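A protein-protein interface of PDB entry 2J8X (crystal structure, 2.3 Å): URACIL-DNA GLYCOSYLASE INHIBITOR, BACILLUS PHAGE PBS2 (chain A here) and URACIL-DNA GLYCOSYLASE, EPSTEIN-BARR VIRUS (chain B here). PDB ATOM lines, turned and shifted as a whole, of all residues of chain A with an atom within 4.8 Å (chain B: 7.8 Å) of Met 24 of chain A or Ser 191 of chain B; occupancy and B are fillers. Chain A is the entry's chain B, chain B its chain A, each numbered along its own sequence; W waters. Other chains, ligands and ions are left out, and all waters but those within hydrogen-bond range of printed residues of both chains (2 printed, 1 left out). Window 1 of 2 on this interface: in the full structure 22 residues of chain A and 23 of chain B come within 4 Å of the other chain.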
ATOM      1  N   GLU A  20     -25.198  -8.758 -24.802  1.00  0.00           N
ATOM      2  CA  GLU A  20     -24.806  -8.543 -23.412  1.00  0.00           C
ATOM      3  C   GLU A  20     -23.480  -7.804 -23.323  1.00  0.00           C
ATOM      4  O   GLU A  20     -22.646  -7.877 -24.232  1.00  0.00           O
ATOM      5  CB  GLU A  20     -24.706  -9.872 -22.656  1.00  0.00           C
ATOM      6  CG  GLU A  20     -23.548 -10.749 -23.112  1.00  0.00           C
ATOM      7  CD  GLU A  20     -23.627 -12.156 -22.557  1.00  0.00           C
ATOM      8  OE1 GLU A  20     -24.752 -12.639 -22.308  1.00  0.00           O
ATOM      9  OE2 GLU A  20     -22.562 -12.783 -22.373  1.00  0.00           O
ATOM     10  N   ILE A  22     -20.669  -7.750 -20.389  1.00  0.00           N
ATOM     11  CA  ILE A  22     -20.247  -8.303 -19.102  1.00  0.00           C
ATOM     12  C   ILE A  22     -18.969  -7.644 -18.589  1.00  0.00           C
ATOM     13  O   ILE A  22     -17.947  -7.621 -19.284  1.00  0.00           O
ATOM     14  CB  ILE A  22     -20.039  -9.834 -19.188  1.00  0.00           C
ATOM     15  CG1 ILE A  22     -21.317 -10.519 -19.680  1.00  0.00           C
ATOM     16  CG2 ILE A  22     -19.589 -10.406 -17.843  1.00  0.00           C
ATOM     17  CD1 ILE A  22     -22.543 -10.263 -18.809  1.00  0.00           C
ATOM     18  N   LEU A  23     -19.033  -7.113 -17.371  1.00  0.00           N
ATOM     19  CA  LEU A  23     -17.870  -6.491 -16.749  1.00  0.00           C
ATOM     20  C   LEU A  23     -16.925  -7.536 -16.178  1.00  0.00           C
ATOM     21  O   LEU A  23     -17.348  -8.447 -15.461  1.00  0.00           O
ATOM     22  CB  LEU A  23     -18.287  -5.511 -15.650  1.00  0.00           C
ATOM     23  CG  LEU A  23     -17.178  -4.597 -15.117  1.00  0.00           C
ATOM     24  CD1 LEU A  23     -16.829  -3.517 -16.127  1.00  0.00           C
ATOM     25  CD2 LEU A  23     -17.577  -3.968 -13.795  1.00  0.00           C
ATOM     26  N   MET A  24     -15.642  -7.390 -16.492  1.00  0.00           N
ATOM     27  CA  MET A  24     -14.616  -8.286 -15.981  1.00  0.00           C
ATOM     28  C   MET A  24     -13.430  -7.513 -15.425  1.00  0.00           C
ATOM     29  O   MET A  24     -13.165  -6.377 -15.837  1.00  0.00           O
ATOM     30  CB  MET A  24     -14.163  -9.263 -17.065  1.00  0.00           C
ATOM     31  CG  MET A  24     -15.242 -10.266 -17.450  1.00  0.00           C
ATOM     32  SD  MET A  24     -14.636 -11.581 -18.517  1.00  0.00           S
ATOM     33  CE  MET A  24     -16.173 -12.350 -19.009  1.00  0.00           C
ATOM     34  N   LEU A  25     -12.726  -8.126 -14.478  1.00  0.00           N
ATOM     35  CA  LEU A  25     -11.545  -7.509 -13.895  1.00  0.00           C
ATOM     36  C   LEU A  25     -10.298  -7.872 -14.708  1.00  0.00           C
ATOM     37  O   LEU A  25     -10.302  -8.856 -15.448  1.00  0.00           O
ATOM     38  CB  LEU A  25     -11.394  -7.908 -12.421  1.00  0.00           C
ATOM     39  CG  LEU A  25     -12.631  -7.672 -11.540  1.00  0.00           C
ATOM     40  CD1 LEU A  25     -12.299  -7.869 -10.069  1.00  0.00           C
ATOM     41  CD2 LEU A  25     -13.240  -6.288 -11.768  1.00  0.00           C
ATOM     42  N   PRO A  26      -9.232  -7.069 -14.578  1.00  0.00           N
ATOM     43  CA  PRO A  26      -8.040  -7.207 -15.407  1.00  0.00           C
ATOM     44  C   PRO A  26      -7.423  -8.601 -15.361  1.00  0.00           C
ATOM     45  O   PRO A  26      -6.983  -9.111 -16.387  1.00  0.00           O
ATOM     46  CB  PRO A  26      -7.079  -6.175 -14.804  1.00  0.00           C
ATOM     47  CG  PRO A  26      -7.970  -5.156 -14.188  1.00  0.00           C
ATOM     48  CD  PRO A  26      -9.105  -5.955 -13.622  1.00  0.00           C
ATOM     49  N   GLU A  28      -8.844 -11.676 -14.706  1.00  0.00           N
ATOM     50  CA  GLU A  28      -9.600 -12.731 -15.389  1.00  0.00           C
ATOM     51  C   GLU A  28      -9.608 -12.526 -16.911  1.00  0.00           C
ATOM     52  O   GLU A  28      -9.710 -13.481 -17.676  1.00  0.00           O
ATOM     53  CB  GLU A  28     -11.027 -12.883 -14.815  1.00  0.00           C
ATOM     54  CG  GLU A  28     -11.909 -11.636 -14.917  1.00  0.00           C
ATOM     55  CD  GLU A  28     -13.175 -11.707 -14.051  1.00  0.00           C
ATOM     56  OE1 GLU A  28     -13.751 -10.634 -13.775  1.00  0.00           O
ATOM     57  OE2 GLU A  28     -13.600 -12.820 -13.651  1.00  0.00           O
ATOM     58  N   VAL A  29      -9.482 -11.276 -17.342  1.00  0.00           N
ATOM     59  CA  VAL A  29      -9.338 -10.964 -18.760  1.00  0.00           C
ATOM     60  C   VAL A  29      -7.971 -11.430 -19.272  1.00  0.00           C
ATOM     61  O   VAL A  29      -7.879 -12.084 -20.312  1.00  0.00           O
ATOM     62  CB  VAL A  29      -9.520  -9.448 -19.019  1.00  0.00           C
ATOM     63  CG1 VAL A  29      -9.154  -9.094 -20.455  1.00  0.00           C
ATOM     64  CG2 VAL A  29     -10.956  -9.019 -18.703  1.00  0.00           C
ATOM     65  N   ASP A  40     -10.956  -2.233 -15.416  1.00  0.00           N
ATOM     66  CA  ASP A  40     -12.050  -3.158 -15.720  1.00  0.00           C
ATOM     67  C   ASP A  40     -12.379  -3.176 -17.215  1.00  0.00           C
ATOM     68  O   ASP A  40     -12.126  -2.206 -17.932  1.00  0.00           O
ATOM     69  CB  ASP A  40     -13.298  -2.813 -14.900  1.00  0.00           C
ATOM     70  CG  ASP A  40     -13.055  -2.883 -13.399  1.00  0.00           C
ATOM     71  OD1 ASP A  40     -12.154  -3.627 -12.970  1.00  0.00           O
ATOM     72  OD2 ASP A  40     -13.768  -2.191 -12.642  1.00  0.00           O
ATOM     73  N   ILE A  41     -12.940  -4.287 -17.679  1.00  0.00           N
ATOM     74  CA  ILE A  41     -13.257  -4.455 -19.095  1.00  0.00           C
ATOM     75  C   ILE A  41     -14.696  -4.906 -19.279  1.00  0.00           C
ATOM     76  O   ILE A  41     -15.147  -5.845 -18.626  1.00  0.00           O
ATOM     77  CB  ILE A  41     -12.320  -5.497 -19.771  1.00  0.00           C
ATOM     78  CG1 ILE A  41     -10.908  -4.931 -19.951  1.00  0.00           C
ATOM     79  CG2 ILE A  41     -12.892  -5.961 -21.111  1.00  0.00           C
ATOM     80  CD1 ILE A  41     -10.762  -3.941 -21.091  1.00  0.00           C
ATOM     81  N   VAL A  43     -17.162  -6.810 -21.627  1.00  0.00           N
ATOM     82  CA  VAL A  43     -17.165  -7.785 -22.710  1.00  0.00           C
ATOM     83  C   VAL A  43     -18.500  -7.747 -23.449  1.00  0.00           C
ATOM     84  O   VAL A  43     -19.459  -8.417 -23.066  1.00  0.00           O
ATOM     85  CB  VAL A  43     -16.882  -9.207 -22.195  1.00  0.00           C
ATOM     86  CG1 VAL A  43     -16.850 -10.199 -23.353  1.00  0.00           C
ATOM     87  CG2 VAL A  43     -15.567  -9.237 -21.419  1.00  0.00           C
ATOM     88  N   GLN B  66     -25.114  -8.449 -13.015  1.00  0.00           N
ATOM     89  CA  GLN B  66     -24.516  -7.133 -12.818  1.00  0.00           C
ATOM     90  C   GLN B  66     -25.571  -6.046 -12.997  1.00  0.00           C
ATOM     91  O   GLN B  66     -26.186  -5.619 -12.028  1.00  0.00           O
ATOM     92  CB  GLN B  66     -23.309  -6.919 -13.752  1.00  0.00           C
ATOM     93  CG  GLN B  66     -22.028  -7.594 -13.250  1.00  0.00           C
ATOM     94  CD  GLN B  66     -21.006  -7.885 -14.348  1.00  0.00           C
ATOM     95  OE1 GLN B  66     -21.126  -7.406 -15.473  1.00  0.00           O
ATOM     96  NE2 GLN B  66     -19.996  -8.678 -14.017  1.00  0.00           N
ATOM     97  N   PHE B  79     -30.153 -12.243 -16.077  1.00  0.00           N
ATOM     98  CA  PHE B  79     -29.890 -13.253 -17.125  1.00  0.00           C
ATOM     99  C   PHE B  79     -31.048 -13.566 -18.079  1.00  0.00           C
ATOM    100  O   PHE B  79     -30.834 -13.819 -19.268  1.00  0.00           O
ATOM    101  CB  PHE B  79     -29.299 -14.538 -16.525  1.00  0.00           C
ATOM    102  CG  PHE B  79     -27.904 -14.361 -15.999  1.00  0.00           C
ATOM    103  CD1 PHE B  79     -27.657 -14.334 -14.634  1.00  0.00           C
ATOM    104  CD2 PHE B  79     -26.836 -14.188 -16.876  1.00  0.00           C
ATOM    105  CE1 PHE B  79     -26.366 -14.151 -14.152  1.00  0.00           C
ATOM    106  CE2 PHE B  79     -25.543 -14.004 -16.398  1.00  0.00           C
ATOM    107  CZ  PHE B  79     -25.312 -13.987 -15.032  1.00  0.00           C
ATOM    108  N   PRO B  89     -25.633 -14.913 -25.054  1.00  0.00           N
ATOM    109  CA  PRO B  89     -24.461 -15.787 -24.931  1.00  0.00           C
ATOM    110  C   PRO B  89     -24.245 -16.417 -23.544  1.00  0.00           C
ATOM    111  O   PRO B  89     -24.041 -17.627 -23.450  1.00  0.00           O
ATOM    112  CB  PRO B  89     -23.304 -14.856 -25.307  1.00  0.00           C
ATOM    113  CG  PRO B  89     -23.928 -13.902 -26.282  1.00  0.00           C
ATOM    114  CD  PRO B  89     -25.292 -13.636 -25.708  1.00  0.00           C
ATOM    115  N   SER B  90     -24.291 -15.616 -22.482  1.00  0.00           N
ATOM    116  CA  SER B  90     -24.086 -16.151 -21.133  1.00  0.00           C
ATOM    117  C   SER B  90     -25.178 -17.145 -20.753  1.00  0.00           C
ATOM    118  O   SER B  90     -24.891 -18.191 -20.180  1.00  0.00           O
ATOM    119  CB  SER B  90     -24.015 -15.032 -20.093  1.00  0.00           C
ATOM    120  OG  SER B  90     -22.820 -14.285 -20.221  1.00  0.00           O
ATOM    121  N   LEU B  91     -26.425 -16.813 -21.078  1.00  0.00           N
ATOM    122  CA  LEU B  91     -27.557 -17.697 -20.795  1.00  0.00           C
ATOM    123  C   LEU B  91     -27.465 -19.002 -21.585  1.00  0.00           C
ATOM    124  O   LEU B  91     -27.721 -20.080 -21.049  1.00  0.00           O
ATOM    125  CB  LEU B  91     -28.887 -16.991 -21.074  1.00  0.00           C
ATOM    126  CG  LEU B  91     -30.129 -17.725 -20.561  1.00  0.00           C
ATOM    127  CD1 LEU B  91     -29.939 -18.158 -19.109  1.00  0.00           C
ATOM    128  CD2 LEU B  91     -31.373 -16.847 -20.696  1.00  0.00           C
ATOM    129  N   ASN B  93     -24.804 -20.346 -22.338  1.00  0.00           N
ATOM    130  CA  ASN B  93     -23.766 -21.100 -21.634  1.00  0.00           C
ATOM    131  C   ASN B  93     -24.244 -21.684 -20.309  1.00  0.00           C
ATOM    132  O   ASN B  93     -23.805 -22.765 -19.905  1.00  0.00           O
ATOM    133  CB  ASN B  93     -22.505 -20.249 -21.455  1.00  0.00           C
ATOM    134  CG  ASN B  93     -21.697 -20.143 -22.742  1.00  0.00           C
ATOM    135  OD1 ASN B  93     -21.938 -20.886 -23.693  1.00  0.00           O
ATOM    136  ND2 ASN B  93     -20.736 -19.224 -22.776  1.00  0.00           N
ATOM    137  N   ILE B  94     -25.149 -20.964 -19.646  1.00  0.00           N
ATOM    138  CA  ILE B  94     -25.835 -21.471 -18.463  1.00  0.00           C
ATOM    139  C   ILE B  94     -26.659 -22.696 -18.837  1.00  0.00           C
ATOM    140  O   ILE B  94     -26.659 -23.689 -18.115  1.00  0.00           O
ATOM    141  CB  ILE B  94     -26.742 -20.390 -17.820  1.00  0.00           C
ATOM    142  CG1 ILE B  94     -25.895 -19.295 -17.181  1.00  0.00           C
ATOM    143  CG2 ILE B  94     -27.680 -20.991 -16.770  1.00  0.00           C
ATOM    144  CD1 ILE B  94     -26.665 -18.010 -16.921  1.00  0.00           C
ATOM    145  N   TRP B 166     -20.733 -15.813 -10.009  1.00  0.00           N
ATOM    146  CA  TRP B 166     -19.996 -16.110 -11.240  1.00  0.00           C
ATOM    147  C   TRP B 166     -19.109 -14.960 -11.677  1.00  0.00           C
ATOM    148  O   TRP B 166     -19.591 -13.891 -12.023  1.00  0.00           O
ATOM    149  CB  TRP B 166     -20.949 -16.497 -12.376  1.00  0.00           C
ATOM    150  CG  TRP B 166     -21.800 -17.695 -12.064  1.00  0.00           C
ATOM    151  CD1 TRP B 166     -21.444 -18.789 -11.326  1.00  0.00           C
ATOM    152  CD2 TRP B 166     -23.147 -17.927 -12.503  1.00  0.00           C
ATOM    153  NE1 TRP B 166     -22.492 -19.683 -11.270  1.00  0.00           N
ATOM    154  CE2 TRP B 166     -23.547 -19.176 -11.982  1.00  0.00           C
ATOM    155  CE3 TRP B 166     -24.056 -17.195 -13.276  1.00  0.00           C
ATOM    156  CZ2 TRP B 166     -24.814 -19.710 -12.214  1.00  0.00           C
ATOM    157  CZ3 TRP B 166     -25.314 -17.729 -13.506  1.00  0.00           C
ATOM    158  CH2 TRP B 166     -25.678 -18.974 -12.983  1.00  0.00           C
ATOM    159  N   GLY B 167     -17.804 -15.191 -11.667  1.00  0.00           N
ATOM    160  CA  GLY B 167     -16.856 -14.159 -12.058  1.00  0.00           C
ATOM    161  C   GLY B 167     -16.337 -13.400 -10.859  1.00  0.00           C
ATOM    162  O   GLY B 167     -16.921 -13.449  -9.774  1.00  0.00           O
ATOM    163  N   ALA B 168     -15.235 -12.689 -11.053  1.00  0.00           N
ATOM    164  CA  ALA B 168     -14.566 -12.031  -9.941  1.00  0.00           C
ATOM    165  C   ALA B 168     -15.397 -10.884  -9.386  1.00  0.00           C
ATOM    166  O   ALA B 168     -15.359 -10.605  -8.190  1.00  0.00           O
ATOM    167  CB  ALA B 168     -13.179 -11.548 -10.355  1.00  0.00           C
ATOM    168  N   LYS B 169     -16.148 -10.221 -10.254  1.00  0.00           N
ATOM    169  CA  LYS B 169     -16.975  -9.100  -9.831  1.00  0.00           C
ATOM    170  C   LYS B 169     -18.137  -9.535  -8.930  1.00  0.00           C
ATOM    171  O   LYS B 169     -18.395  -8.906  -7.905  1.00  0.00           O
ATOM    172  CB  LYS B 169     -17.440  -8.283 -11.043  1.00  0.00           C
ATOM    173  CG  LYS B 169     -18.760  -7.579 -10.852  1.00  0.00           C
ATOM    174  CD  LYS B 169     -18.724  -6.157 -11.359  1.00  0.00           C
ATOM    175  CE  LYS B 169     -18.200  -5.221 -10.278  1.00  0.00           C
ATOM    176  NZ  LYS B 169     -18.653  -3.820 -10.498  1.00  0.00           N
ATOM    177  N   GLN B 188     -15.813 -18.992 -12.810  1.00  0.00           N
ATOM    178  CA  GLN B 188     -15.782 -17.926 -13.797  1.00  0.00           C
ATOM    179  C   GLN B 188     -17.193 -17.620 -14.287  1.00  0.00           C
ATOM    180  O   GLN B 188     -18.105 -18.434 -14.134  1.00  0.00           O
ATOM    181  CB  GLN B 188     -14.890 -18.316 -14.979  1.00  0.00           C
ATOM    182  CG  GLN B 188     -13.416 -18.367 -14.647  1.00  0.00           C
ATOM    183  CD  GLN B 188     -12.603 -18.996 -15.758  1.00  0.00           C
ATOM    184  OE1 GLN B 188     -13.152 -19.491 -16.739  1.00  0.00           O
ATOM    185  NE2 GLN B 188     -11.292 -18.982 -15.609  1.00  0.00           N
ATOM    186  N   HIS B 189     -17.360 -16.438 -14.871  1.00  0.00           N
ATOM    187  CA  HIS B 189     -18.630 -16.010 -15.444  1.00  0.00           C
ATOM    188  C   HIS B 189     -18.989 -16.915 -16.624  1.00  0.00           C
ATOM    189  O   HIS B 189     -18.104 -17.456 -17.265  1.00  0.00           O
ATOM    190  CB  HIS B 189     -18.513 -14.551 -15.903  1.00  0.00           C
ATOM    191  CG  HIS B 189     -19.822 -13.923 -16.269  1.00  0.00           C
ATOM    192  ND1 HIS B 189     -20.554 -13.162 -15.383  1.00  0.00           N
ATOM    193  CD2 HIS B 189     -20.534 -13.955 -17.419  1.00  0.00           C
ATOM    194  CE1 HIS B 189     -21.663 -12.753 -15.972  1.00  0.00           C
ATOM    195  NE2 HIS B 189     -21.675 -13.216 -17.208  1.00  0.00           N
ATOM    196  N   PRO B 190     -20.292 -17.105 -16.894  1.00  0.00           N
ATOM    197  CA  PRO B 190     -20.733 -17.887 -18.064  1.00  0.00           C
ATOM    198  C   PRO B 190     -20.452 -17.251 -19.436  1.00  0.00           C
ATOM    199  O   PRO B 190     -20.711 -17.878 -20.464  1.00  0.00           O
ATOM    200  CB  PRO B 190     -22.242 -18.034 -17.841  1.00  0.00           C
ATOM    201  CG  PRO B 190     -22.605 -16.904 -16.949  1.00  0.00           C
ATOM    202  CD  PRO B 190     -21.429 -16.650 -16.073  1.00  0.00           C
ATOM    203  N   SER B 191     -19.929 -16.030 -19.451  1.00  0.00           N
ATOM    204  CA  SER B 191     -19.517 -15.371 -20.698  1.00  0.00           C
ATOM    205  C   SER B 191     -18.615 -16.253 -21.564  1.00  0.00           C
ATOM    206  O   SER B 191     -17.689 -16.889 -21.057  1.00  0.00           O
ATOM    207  CB  SER B 191     -18.788 -14.063 -20.389  1.00  0.00           C
ATOM    208  OG  SER B 191     -18.213 -13.508 -21.558  1.00  0.00           O
ATOM    209  N   PRO B 192     -18.871 -16.279 -22.885  1.00  0.00           N
ATOM    210  CA  PRO B 192     -18.070 -17.086 -23.812  1.00  0.00           C
ATOM    211  C   PRO B 192     -16.569 -16.797 -23.736  1.00  0.00           C
ATOM    212  O   PRO B 192     -15.765 -17.660 -24.093  1.00  0.00           O
ATOM    213  CB  PRO B 192     -18.606 -16.676 -25.189  1.00  0.00           C
ATOM    214  CG  PRO B 192     -19.988 -16.187 -24.925  1.00  0.00           C
ATOM    215  CD  PRO B 192     -19.941 -15.538 -23.576  1.00  0.00           C
ATOM    216  N   LEU B 193     -16.193 -15.602 -23.288  1.00  0.00           N
ATOM    217  CA  LEU B 193     -14.781 -15.213 -23.253  1.00  0.00           C
ATOM    218  C   LEU B 193     -13.964 -16.140 -22.364  1.00  0.00           C
ATOM    219  O   LEU B 193     -12.936 -16.678 -22.787  1.00  0.00           O
ATOM    220  CB  LEU B 193     -14.605 -13.764 -22.777  1.00  0.00           C
ATOM    221  CG  LEU B 193     -13.154 -13.262 -22.799  1.00  0.00           C
ATOM    222  CD1 LEU B 193     -12.679 -12.996 -24.228  1.00  0.00           C
ATOM    223  CD2 LEU B 193     -12.978 -12.018 -21.944  1.00  0.00           C
ATOM    224  N   ALA B 194     -14.433 -16.317 -21.135  1.00  0.00           N
ATOM    225  CA  ALA B 194     -13.741 -17.122 -20.131  1.00  0.00           C
ATOM    226  C   ALA B 194     -13.416 -18.543 -20.597  1.00  0.00           C
ATOM    227  O   ALA B 194     -12.484 -19.170 -20.085  1.00  0.00           O
ATOM    228  CB  ALA B 194     -14.554 -17.155 -18.828  1.00  0.00           C
ATOM    229  N   GLN B 195     -14.176 -19.047 -21.563  1.00  0.00           N
ATOM    230  CA  GLN B 195     -13.983 -20.417 -22.059  1.00  0.00           C
ATOM    231  C   GLN B 195     -12.549 -20.723 -22.515  1.00  0.00           C
ATOM    232  O   GLN B 195     -12.078 -21.862 -22.396  1.00  0.00           O
ATOM    233  CB  GLN B 195     -14.972 -20.730 -23.189  1.00  0.00           C
ATOM    234  CG  GLN B 195     -16.424 -20.801 -22.741  1.00  0.00           C
ATOM    235  CD  GLN B 195     -17.303 -21.553 -23.720  1.00  0.00           C
ATOM    236  OE1 GLN B 195     -17.024 -21.594 -24.920  1.00  0.00           O
ATOM    237  NE2 GLN B 195     -18.374 -22.155 -23.212  1.00  0.00           N
ATOM    238  N   ASN B 196     -11.865 -19.707 -23.039  1.00  0.00           N
ATOM    239  CA  ASN B 196     -10.509 -19.888 -23.563  1.00  0.00           C
ATOM    240  C   ASN B 196      -9.418 -19.392 -22.610  1.00  0.00           C
ATOM    241  O   ASN B 196      -8.272 -19.199 -23.013  1.00  0.00           O
ATOM    242  CB  ASN B 196     -10.368 -19.230 -24.943  1.00  0.00           C
ATOM    243  CG  ASN B 196     -11.195 -19.932 -26.015  1.00  0.00           C
ATOM    244  OD1 ASN B 196     -12.337 -19.553 -26.278  1.00  0.00           O
ATOM    245  ND2 ASN B 196     -10.624 -20.965 -26.629  1.00  0.00           N
ATOM    246  N   PHE B 206     -16.640 -22.089 -15.947  1.00  0.00           N
ATOM    247  CA  PHE B 206     -18.075 -22.143 -15.696  1.00  0.00           C
ATOM    248  C   PHE B 206     -18.653 -23.468 -16.191  1.00  0.00           C
ATOM    249  O   PHE B 206     -19.386 -24.149 -15.473  1.00  0.00           O
ATOM    250  CB  PHE B 206     -18.815 -20.978 -16.369  1.00  0.00           C
ATOM    251  CG  PHE B 206     -20.313 -21.029 -16.172  1.00  0.00           C
ATOM    252  CD1 PHE B 206     -20.904 -20.393 -15.094  1.00  0.00           C
ATOM    253  CD2 PHE B 206     -21.122 -21.739 -17.050  1.00  0.00           C
ATOM    254  CE1 PHE B 206     -22.285 -20.458 -14.892  1.00  0.00           C
ATOM    255  CE2 PHE B 206     -22.506 -21.809 -16.851  1.00  0.00           C
ATOM    256  CZ  PHE B 206     -23.082 -21.165 -15.769  1.00  0.00           C
HETATM  257  O   HOH W   1     -16.505 -10.636 -13.691  1.00  0.00           O
HETATM  258  O   HOH W   2     -14.892 -14.839 -15.284  1.00  0.00           O
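The side-chain amide oxygen (OE1) of Gln 66 of chain B is in hydrogen-bond range of the backbone NH (N) of Leu 23 of chain A (2.8 Å). OE2 of Glu 20 of chain A lies within hydrogen-bond range of OG of Ser 90 of chain B (2.6 Å). The backbone NH of Ala 168 of chain B is in hydrogen-bond range of the side-chain carboxylate of Glu 28 of chain A (3.1 Å).
The backbone NH of Leu 193 of chain B sits close to the side-chain hydroxyl of Ser 191 of chain B. The backbone carbonyl oxygen (O) of Ile 22 of chain A sits at hydrogen-bond distance from the backbone NH (N) of Val 43 of chain A. The side-chain hydroxyl (OG) of Ser 90 of chain B sits at hydrogen-bond distance from the backbone NH (N) of Ser 191 of chain B (3.5 Å). N of Leu 25 of chain A sits at hydrogen-bond distance from OE1 of Glu 28 of chain A, at 2.8 Å. A ring nitrogen (NE2) of His 189 of chain B sits at hydrogen-bond distance from the side-chain hydroxyl (OG) of Ser 90 of chain B, 3.4 Å away. The backbone NH (N) of Met 24 of chain A sits at hydrogen-bond distance from the backbone carbonyl oxygen (O) of Ile 41 of chain A (2.7 Å).
Among the printed residues, pairs that only touch across the chains: Glu 20 of chain A with Pro 89 of chain B, Glu 20 of chain A with Pro 192 of chain B, Ile 22 of chain A with Gln 66 of chain B, Ile 22 of chain A with His 189 of chain B, Leu 23 of chain A with Lys 169 of chain B, Met 24 of chain A with Ser 191 of chain B, Met 24 of chain A with Leu 193 of chain B, Leu 25 of chain A with Ala 168 of chain B, Glu 28 of chain A with Gly 167 of chain B and Val 43 of chain A with Leu 193 of chain B.
Of the printed residues of chain A, Ser 191 of chain B touches Met 24 (3.4 Å). Printed residues of chain B within 4 Å of Ile 22 of chain A: Gln 66 and His 189. Printed residues of chain A within 4 Å of Ser 90 of chain B: Glu 20 (2.6 Å). Of the printed residues of chain B, Leu 23 of chain A touches Gln 66 (2.8 Å) and Lys 169 (3.5 Å). Of the printed residues of chain A, Gly 167 of chain B touches Glu 28. Val 29 of chain A touches none of the printed residues of chain B. The nearest residue of chain B that does not touch Met 24 of chain A is His 189 of chain B (4.5 Å). The nearest printed residue of chain A that does not touch Ser 191 of chain B is Val 43 of chain A (4.004 Å). The nearest printed residue of chain B that does not touch Leu 23 of chain A is His 189 of chain B (5.7 Å).
Hydrophobic or aromatic side chains of chain A that line the printed part of chain B: Ile 22, Leu 23, Met 24, Leu 25 and Val 43. Of the 21 printed residues of chain B, 10 touch a printed residue of chain A. Hydrophobic or aromatic side chains of chain B that line the printed part of chain A: Pro 89, Ala 168, His 189, Pro 192 and Leu 193. Among the printed residues, 13 pairs touch across the chains. Among the printed residues, no Asp or Glu carboxylate lies within 4 Å of a Lys or Arg side-chain nitrogen of the other chain.
Water W1 lies within hydrogen-bond range of OE1 of Glu 28 of chain A, O of Leu 23 of chain A and N of Lys 169 of chain B. Water W2 bridges OE2 of Glu 28 of chain A (2.9 Å) and N of His 189 of chain B (3.0 Å).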
